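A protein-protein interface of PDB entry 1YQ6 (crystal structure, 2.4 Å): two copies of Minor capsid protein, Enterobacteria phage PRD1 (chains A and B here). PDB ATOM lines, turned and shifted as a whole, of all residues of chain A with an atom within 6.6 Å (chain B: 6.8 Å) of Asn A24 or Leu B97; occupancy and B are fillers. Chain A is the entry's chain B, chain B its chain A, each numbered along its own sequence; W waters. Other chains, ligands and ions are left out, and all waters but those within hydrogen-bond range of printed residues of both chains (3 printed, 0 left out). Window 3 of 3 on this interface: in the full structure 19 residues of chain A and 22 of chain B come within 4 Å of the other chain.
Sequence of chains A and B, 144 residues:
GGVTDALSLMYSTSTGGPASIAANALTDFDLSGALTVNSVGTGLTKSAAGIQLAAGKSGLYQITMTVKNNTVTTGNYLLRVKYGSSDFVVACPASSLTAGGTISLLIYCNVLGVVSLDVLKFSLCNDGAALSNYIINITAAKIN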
ATOM      1  N   ILE A  21     -36.978 -21.591   7.091  1.00  0.00           N
ATOM      2  CA  ILE A  21     -36.137 -22.690   6.643  1.00  0.00           C
ATOM      3  C   ILE A  21     -35.318 -23.114   7.847  1.00  0.00           C
ATOM      4  O   ILE A  21     -34.491 -22.348   8.342  1.00  0.00           O
ATOM      5  CB  ILE A  21     -35.211 -22.254   5.484  1.00  0.00           C
ATOM      6  CG1 ILE A  21     -36.054 -21.827   4.286  1.00  0.00           C
ATOM      7  CG2 ILE A  21     -34.308 -23.402   5.069  1.00  0.00           C
ATOM      8  CD1 ILE A  21     -35.246 -21.259   3.131  1.00  0.00           C
ATOM      9  N   ALA A  22     -35.571 -24.332   8.323  1.00  0.00           N
ATOM     10  CA  ALA A  22     -34.897 -24.874   9.499  1.00  0.00           C
ATOM     11  C   ALA A  22     -33.386 -24.836   9.393  1.00  0.00           C
ATOM     12  O   ALA A  22     -32.826 -24.966   8.305  1.00  0.00           O
ATOM     13  CB  ALA A  22     -35.358 -26.302   9.742  1.00  0.00           C
ATOM     14  N   ALA A  23     -32.732 -24.672  10.535  1.00  0.00           N
ATOM     15  CA  ALA A  23     -31.285 -24.620  10.599  1.00  0.00           C
ATOM     16  C   ALA A  23     -30.655 -26.005  10.448  1.00  0.00           C
ATOM     17  O   ALA A  23     -31.270 -27.028  10.781  1.00  0.00           O
ATOM     18  CB  ALA A  23     -30.853 -24.004  11.919  1.00  0.00           C
ATOM     19  N   ASN A  24     -29.424 -26.021   9.936  1.00  0.00           N
ATOM     20  CA  ASN A  24     -28.653 -27.244   9.754  1.00  0.00           C
ATOM     21  C   ASN A  24     -29.427 -28.468   9.269  1.00  0.00           C
ATOM     22  O   ASN A  24     -29.376 -29.534   9.889  1.00  0.00           O
ATOM     23  CB  ASN A  24     -27.955 -27.586  11.058  1.00  0.00           C
ATOM     24  CG  ASN A  24     -26.672 -28.328  10.844  1.00  0.00           C
ATOM     25  OD1 ASN A  24     -26.275 -29.126  11.679  1.00  0.00           O
ATOM     26  ND2 ASN A  24     -26.004 -28.062   9.736  1.00  0.00           N
ATOM     27  N   ALA A  25     -30.135 -28.322   8.161  1.00  0.00           N
ATOM     28  CA  ALA A  25     -30.891 -29.431   7.590  1.00  0.00           C
ATOM     29  C   ALA A  25     -31.184 -29.049   6.148  1.00  0.00           C
ATOM     30  O   ALA A  25     -31.219 -27.870   5.823  1.00  0.00           O
ATOM     31  CB  ALA A  25     -32.190 -29.654   8.359  1.00  0.00           C
ATOM     32  N   LEU A  26     -31.369 -30.040   5.285  1.00  0.00           N
ATOM     33  CA  LEU A  26     -31.651 -29.775   3.889  1.00  0.00           C
ATOM     34  C   LEU A  26     -32.900 -30.492   3.405  1.00  0.00           C
ATOM     35  O   LEU A  26     -32.861 -31.677   3.100  1.00  0.00           O
ATOM     36  CB  LEU A  26     -30.461 -30.185   3.019  1.00  0.00           C
ATOM     37  CG  LEU A  26     -29.187 -29.340   3.114  1.00  0.00           C
ATOM     38  CD1 LEU A  26     -28.100 -29.975   2.251  1.00  0.00           C
ATOM     39  CD2 LEU A  26     -29.471 -27.910   2.669  1.00  0.00           C
ATOM     40  N   LEU A  78     -25.443 -23.588   3.417  1.00  0.00           N
ATOM     41  CA  LEU A  78     -25.263 -24.863   2.743  1.00  0.00           C
ATOM     42  C   LEU A  78     -26.225 -24.955   1.576  1.00  0.00           C
ATOM     43  O   LEU A  78     -27.425 -24.798   1.747  1.00  0.00           O
ATOM     44  CB  LEU A  78     -25.523 -26.012   3.726  1.00  0.00           C
ATOM     45  CG  LEU A  78     -24.862 -25.915   5.106  1.00  0.00           C
ATOM     46  CD1 LEU A  78     -25.171 -27.167   5.895  1.00  0.00           C
ATOM     47  CD2 LEU A  78     -23.363 -25.741   4.971  1.00  0.00           C
ATOM     48  N   LEU A  79     -25.702 -25.194   0.382  1.00  0.00           N
ATOM     49  CA  LEU A  79     -26.561 -25.297  -0.792  1.00  0.00           C
ATOM     50  C   LEU A  79     -26.425 -26.652  -1.464  1.00  0.00           C
ATOM     51  O   LEU A  79     -25.344 -27.228  -1.505  1.00  0.00           O
ATOM     52  CB  LEU A  79     -26.241 -24.185  -1.797  1.00  0.00           C
ATOM     53  CG  LEU A  79     -26.575 -22.760  -1.358  1.00  0.00           C
ATOM     54  CD1 LEU A  79     -25.594 -22.309  -0.302  1.00  0.00           C
ATOM     55  CD2 LEU A  79     -26.521 -21.832  -2.553  1.00  0.00           C
ATOM     56  N   ARG A  80     -27.530 -27.157  -1.997  1.00  0.00           N
ATOM     57  CA  ARG A  80     -27.514 -28.452  -2.648  1.00  0.00           C
ATOM     58  C   ARG A  80     -28.453 -28.532  -3.827  1.00  0.00           C
ATOM     59  O   ARG A  80     -29.561 -28.008  -3.786  1.00  0.00           O
ATOM     60  CB  ARG A  80     -27.888 -29.541  -1.646  1.00  0.00           C
ATOM     61  CG  ARG A  80     -27.826 -30.957  -2.208  1.00  0.00           C
ATOM     62  CD  ARG A  80     -28.258 -31.969  -1.172  1.00  0.00           C
ATOM     63  NE  ARG A  80     -29.705 -31.943  -0.987  1.00  0.00           N
ATOM     64  CZ  ARG A  80     -30.329 -32.443   0.074  1.00  0.00           C
ATOM     65  NH1 ARG A  80     -29.627 -33.002   1.051  1.00  0.00           N
ATOM     66  NH2 ARG A  80     -31.649 -32.391   0.155  1.00  0.00           N
ATOM     67  N   ASP A  87     -25.888 -35.668  -6.628  1.00  0.00           N
ATOM     68  CA  ASP A  87     -26.212 -34.497  -5.838  1.00  0.00           C
ATOM     69  C   ASP A  87     -24.941 -33.651  -5.789  1.00  0.00           C
ATOM     70  O   ASP A  87     -23.846 -34.181  -5.764  1.00  0.00           O
ATOM     71  CB  ASP A  87     -26.713 -34.884  -4.439  1.00  0.00           C
ATOM     72  CG  ASP A  87     -25.626 -35.420  -3.561  1.00  0.00           C
ATOM     73  OD1 ASP A  87     -24.920 -36.348  -4.008  1.00  0.00           O
ATOM     74  OD2 ASP A  87     -25.467 -34.918  -2.423  1.00  0.00           O
ATOM     75  N   VAL A  89     -23.003 -30.209  -3.953  1.00  0.00           N
ATOM     76  CA  VAL A  89     -23.061 -29.334  -2.797  1.00  0.00           C
ATOM     77  C   VAL A  89     -21.944 -28.306  -2.708  1.00  0.00           C
ATOM     78  O   VAL A  89     -20.926 -28.399  -3.388  1.00  0.00           O
ATOM     79  CB  VAL A  89     -23.023 -30.161  -1.491  1.00  0.00           C
ATOM     80  CG1 VAL A  89     -24.072 -31.253  -1.529  1.00  0.00           C
ATOM     81  CG2 VAL A  89     -21.640 -30.772  -1.302  1.00  0.00           C
ATOM     82  N   CYS A 125     -29.719 -23.841   3.379  1.00  0.00           N
ATOM     83  CA  CYS A 125     -30.002 -23.495   4.764  1.00  0.00           C
ATOM     84  C   CYS A 125     -28.751 -22.855   5.319  1.00  0.00           C
ATOM     85  O   CYS A 125     -27.770 -22.688   4.605  1.00  0.00           O
ATOM     86  CB  CYS A 125     -30.297 -24.760   5.583  1.00  0.00           C
ATOM     87  SG  CYS A 125     -28.807 -25.706   6.078  1.00  0.00           S
ATOM     88  N   ASN A 126     -28.795 -22.492   6.593  1.00  0.00           N
ATOM     89  CA  ASN A 126     -27.631 -21.954   7.274  1.00  0.00           C
ATOM     90  C   ASN A 126     -27.405 -23.018   8.340  1.00  0.00           C
ATOM     91  O   ASN A 126     -28.373 -23.506   8.916  1.00  0.00           O
ATOM     92  CB  ASN A 126     -27.928 -20.620   7.947  1.00  0.00           C
ATOM     93  CG  ASN A 126     -26.708 -20.048   8.633  1.00  0.00           C
ATOM     94  OD1 ASN A 126     -25.847 -19.445   7.991  1.00  0.00           O
ATOM     95  ND2 ASN A 126     -26.613 -20.253   9.940  1.00  0.00           N
ATOM     96  N   ASP A 127     -26.157 -23.385   8.614  1.00  0.00           N
ATOM     97  CA  ASP A 127     -25.917 -24.437   9.590  1.00  0.00           C
ATOM     98  C   ASP A 127     -26.087 -24.021  11.038  1.00  0.00           C
ATOM     99  O   ASP A 127     -26.033 -24.868  11.932  1.00  0.00           O
ATOM    100  CB  ASP A 127     -24.525 -25.075   9.391  1.00  0.00           C
ATOM    101  CG  ASP A 127     -23.390 -24.088   9.562  1.00  0.00           C
ATOM    102  OD1 ASP A 127     -23.628 -22.962  10.043  1.00  0.00           O
ATOM    103  OD2 ASP A 127     -22.243 -24.443   9.221  1.00  0.00           O
ATOM    104  N   GLY A 128     -26.316 -22.736  11.283  1.00  0.00           N
ATOM    105  CA  GLY A 128     -26.466 -22.290  12.656  1.00  0.00           C
ATOM    106  C   GLY A 128     -27.697 -21.465  12.981  1.00  0.00           C
ATOM    107  O   GLY A 128     -27.891 -21.084  14.133  1.00  0.00           O
ATOM    108  N   ALA A 129     -28.536 -21.184  11.992  1.00  0.00           N
ATOM    109  CA  ALA A 129     -29.721 -20.386  12.244  1.00  0.00           C
ATOM    110  C   ALA A 129     -30.781 -20.621  11.189  1.00  0.00           C
ATOM    111  O   ALA A 129     -30.474 -21.035  10.070  1.00  0.00           O
ATOM    112  CB  ALA A 129     -29.352 -18.926  12.275  1.00  0.00           C
ATOM    113  N   ALA A 130     -32.032 -20.361  11.545  1.00  0.00           N
ATOM    114  CA  ALA A 130     -33.141 -20.534  10.615  1.00  0.00           C
ATOM    115  C   ALA A 130     -33.196 -19.313   9.709  1.00  0.00           C
ATOM    116  O   ALA A 130     -32.740 -18.232  10.085  1.00  0.00           O
ATOM    117  CB  ALA A 130     -34.456 -20.676  11.385  1.00  0.00           C
ATOM    118  N   LYS B  68     -18.116 -35.455  -4.284  1.00  0.00           N
ATOM    119  CA  LYS B  68     -18.846 -35.944  -3.128  1.00  0.00           C
ATOM    120  C   LYS B  68     -17.998 -37.102  -2.620  1.00  0.00           C
ATOM    121  O   LYS B  68     -17.590 -37.971  -3.383  1.00  0.00           O
ATOM    122  CB  LYS B  68     -20.256 -36.458  -3.485  1.00  0.00           C
ATOM    123  CG  LYS B  68     -21.317 -35.387  -3.784  1.00  0.00           C
ATOM    124  CD  LYS B  68     -21.447 -34.344  -2.675  1.00  0.00           C
ATOM    125  CE  LYS B  68     -21.745 -34.952  -1.303  1.00  0.00           C
ATOM    126  NZ  LYS B  68     -23.058 -35.648  -1.237  1.00  0.00           N
ATOM    127  N   THR B  73     -16.216 -35.606   6.117  1.00  0.00           N
ATOM    128  CA  THR B  73     -17.100 -34.489   6.408  1.00  0.00           C
ATOM    129  C   THR B  73     -16.470 -33.350   7.191  1.00  0.00           C
ATOM    130  O   THR B  73     -17.179 -32.502   7.728  1.00  0.00           O
ATOM    131  CB  THR B  73     -18.346 -34.987   7.175  1.00  0.00           C
ATOM    132  OG1 THR B  73     -17.951 -35.469   8.462  1.00  0.00           O
ATOM    133  CG2 THR B  73     -19.010 -36.121   6.422  1.00  0.00           C
ATOM    134  N   ALA B  94     -16.414 -28.453   4.505  1.00  0.00           N
ATOM    135  CA  ALA B  94     -17.085 -29.738   4.558  1.00  0.00           C
ATOM    136  C   ALA B  94     -17.987 -29.861   5.766  1.00  0.00           C
ATOM    137  O   ALA B  94     -17.744 -29.261   6.810  1.00  0.00           O
ATOM    138  CB  ALA B  94     -16.055 -30.858   4.581  1.00  0.00           C
ATOM    139  N   SER B  95     -19.039 -30.646   5.608  1.00  0.00           N
ATOM    140  CA  SER B  95     -19.979 -30.907   6.689  1.00  0.00           C
ATOM    141  C   SER B  95     -20.674 -32.197   6.290  1.00  0.00           C
ATOM    142  O   SER B  95     -20.509 -32.677   5.170  1.00  0.00           O
ATOM    143  CB  SER B  95     -21.007 -29.786   6.828  1.00  0.00           C
ATOM    144  OG  SER B  95     -21.994 -29.880   5.822  1.00  0.00           O
ATOM    145  N   SER B  96     -21.444 -32.759   7.202  1.00  0.00           N
ATOM    146  CA  SER B  96     -22.143 -33.988   6.917  1.00  0.00           C
ATOM    147  C   SER B  96     -23.196 -33.745   5.828  1.00  0.00           C
ATOM    148  O   SER B  96     -23.504 -34.635   5.045  1.00  0.00           O
ATOM    149  CB  SER B  96     -22.785 -34.501   8.202  1.00  0.00           C
ATOM    150  OG  SER B  96     -23.276 -35.805   7.998  1.00  0.00           O
ATOM    151  N   LEU B  97     -23.734 -32.527   5.771  1.00  0.00           N
ATOM    152  CA  LEU B  97     -24.738 -32.172   4.771  1.00  0.00           C
ATOM    153  C   LEU B  97     -24.102 -31.755   3.454  1.00  0.00           C
ATOM    154  O   LEU B  97     -24.734 -31.817   2.405  1.00  0.00           O
ATOM    155  CB  LEU B  97     -25.620 -31.042   5.295  1.00  0.00           C
ATOM    156  CG  LEU B  97     -26.595 -31.484   6.378  1.00  0.00           C
ATOM    157  CD1 LEU B  97     -27.205 -30.286   7.066  1.00  0.00           C
ATOM    158  CD2 LEU B  97     -27.665 -32.349   5.736  1.00  0.00           C
ATOM    159  N   THR B  98     -22.851 -31.322   3.514  1.00  0.00           N
ATOM    160  CA  THR B  98     -22.129 -30.902   2.317  1.00  0.00           C
ATOM    161  C   THR B  98     -20.740 -31.550   2.274  1.00  0.00           C
ATOM    162  O   THR B  98     -19.716 -30.878   2.403  1.00  0.00           O
ATOM    163  CB  THR B  98     -21.984 -29.361   2.266  1.00  0.00           C
ATOM    164  OG1 THR B  98     -21.146 -28.915   3.338  1.00  0.00           O
ATOM    165  CG2 THR B  98     -23.346 -28.696   2.401  1.00  0.00           C
ATOM    166  N   ALA B  99     -20.726 -32.869   2.087  1.00  0.00           N
ATOM    167  CA  ALA B  99     -19.496 -33.655   2.032  1.00  0.00           C
ATOM    168  C   ALA B  99     -18.810 -33.575   0.675  1.00  0.00           C
ATOM    169  O   ALA B  99     -18.648 -34.587  -0.014  1.00  0.00           O
ATOM    170  CB  ALA B  99     -19.810 -35.109   2.364  1.00  0.00           C
ATOM    171  N   GLY B 100     -18.394 -32.377   0.289  1.00  0.00           N
ATOM    172  CA  GLY B 100     -17.743 -32.210  -0.991  1.00  0.00           C
ATOM    173  C   GLY B 100     -17.681 -30.751  -1.362  1.00  0.00           C
ATOM    174  O   GLY B 100     -17.705 -29.895  -0.488  1.00  0.00           O
HETATM  175  O   HOH W   1     -23.845 -38.149  -2.296  1.00  0.00           O
HETATM  176  O   HOH W   2     -26.019 -34.966   0.074  1.00  0.00           O
HETATM  177  O   HOH W   3     -26.774 -33.484   2.134  1.00  0.00           O
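OD2 of Asp A87 lies within salt-bridge range of NZ of Lys B68 (2.8 Å).
The guanidinium group (NH2) of Arg A80 sits at hydrogen-bond distance from the backbone carbonyl oxygen (O) of Leu A26 (3.3 Å). The side-chain hydroxyl (OG1) of Thr B98 sits at hydrogen-bond distance from the side-chain hydroxyl (OG) of Ser B95 (2.8 Å). N of Asn A24 lies within hydrogen-bond range of O of Asn A126 (2.9 Å). The backbone NH of Leu B97 lies close to the side-chain hydroxyl of Ser B95, 3.2 Å away. O of Cys A125 sits at hydrogen-bond distance from N of Leu A78. O of Ala A25 is in hydrogen-bond range of SG of Cys A125, at 3.3 Å.
Asn A24 touches Leu B97 (C to CD1, 3.6 Å). N of Ala A25 touches CD1 of Leu B97, 3.7 Å away. Leu A26 touches Leu B97 (CD1 to O, 3.8 Å). Leu B97 touches Leu A78. CB of Leu A78 touches CG2 of Thr B98, at 3.7 Å. Lys B68 touches Val A89. Val A89 touches Thr B98. CG2 of Val A89 touches N of Gly B100, 3.96 Å away.
Of chain B, only Leu B97 (3.6 Å) comes within 4 Å of Asn A24. Of the printed residues of chain B, Ala A25 touches Leu B97 (3.7 Å). Of the printed residues of chain B, Val A89 touches Lys B68 (3.8 Å), Thr B98 (3.7 Å) and Gly B100 (3.96 Å). Asp A127 touches none of the printed residues of chain B. Of the printed residues of chain A, Thr B98 touches Leu A78 and Val A89. Ala B99 touches none of the printed residues of chain A. Of the printed residues of chain A, Gly B100 touches Val A89. The nearest printed residue of chain B that does not touch Leu A26 is Thr B98 (4.9 Å).
Hydrophobic or aromatic side chains of chain A within 4 Å of the printed part of chain B: Leu A26, Leu A78 and Val A89. Hydrophobic or aromatic side chains of chain B that line the printed part of chain A: Leu B97. Among the printed residues, 9 pairs touch across the chains. Among the printed residues, Asp or Glu carboxylates within 4 Å of a Lys or Arg side-chain nitrogen of the other chain: Asp A87 with Lys B68.
No position is printed for both chains. Of the 9 pairs that touch across the chains among the printed residues, none has its exchanged pair printed and touching as well.
Water W2 lies within hydrogen-bond range of OD2 of Asp A87 (2.6 Å) and NZ of Lys B68 (3.3 Å). Water W3 bridges O of Leu B97 and NH1 of Arg A80. Water W1 lies within hydrogen-bond range of OD1 of Asp A87 (2.7 Å) and NZ of Lys B68 (2.8 Å).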
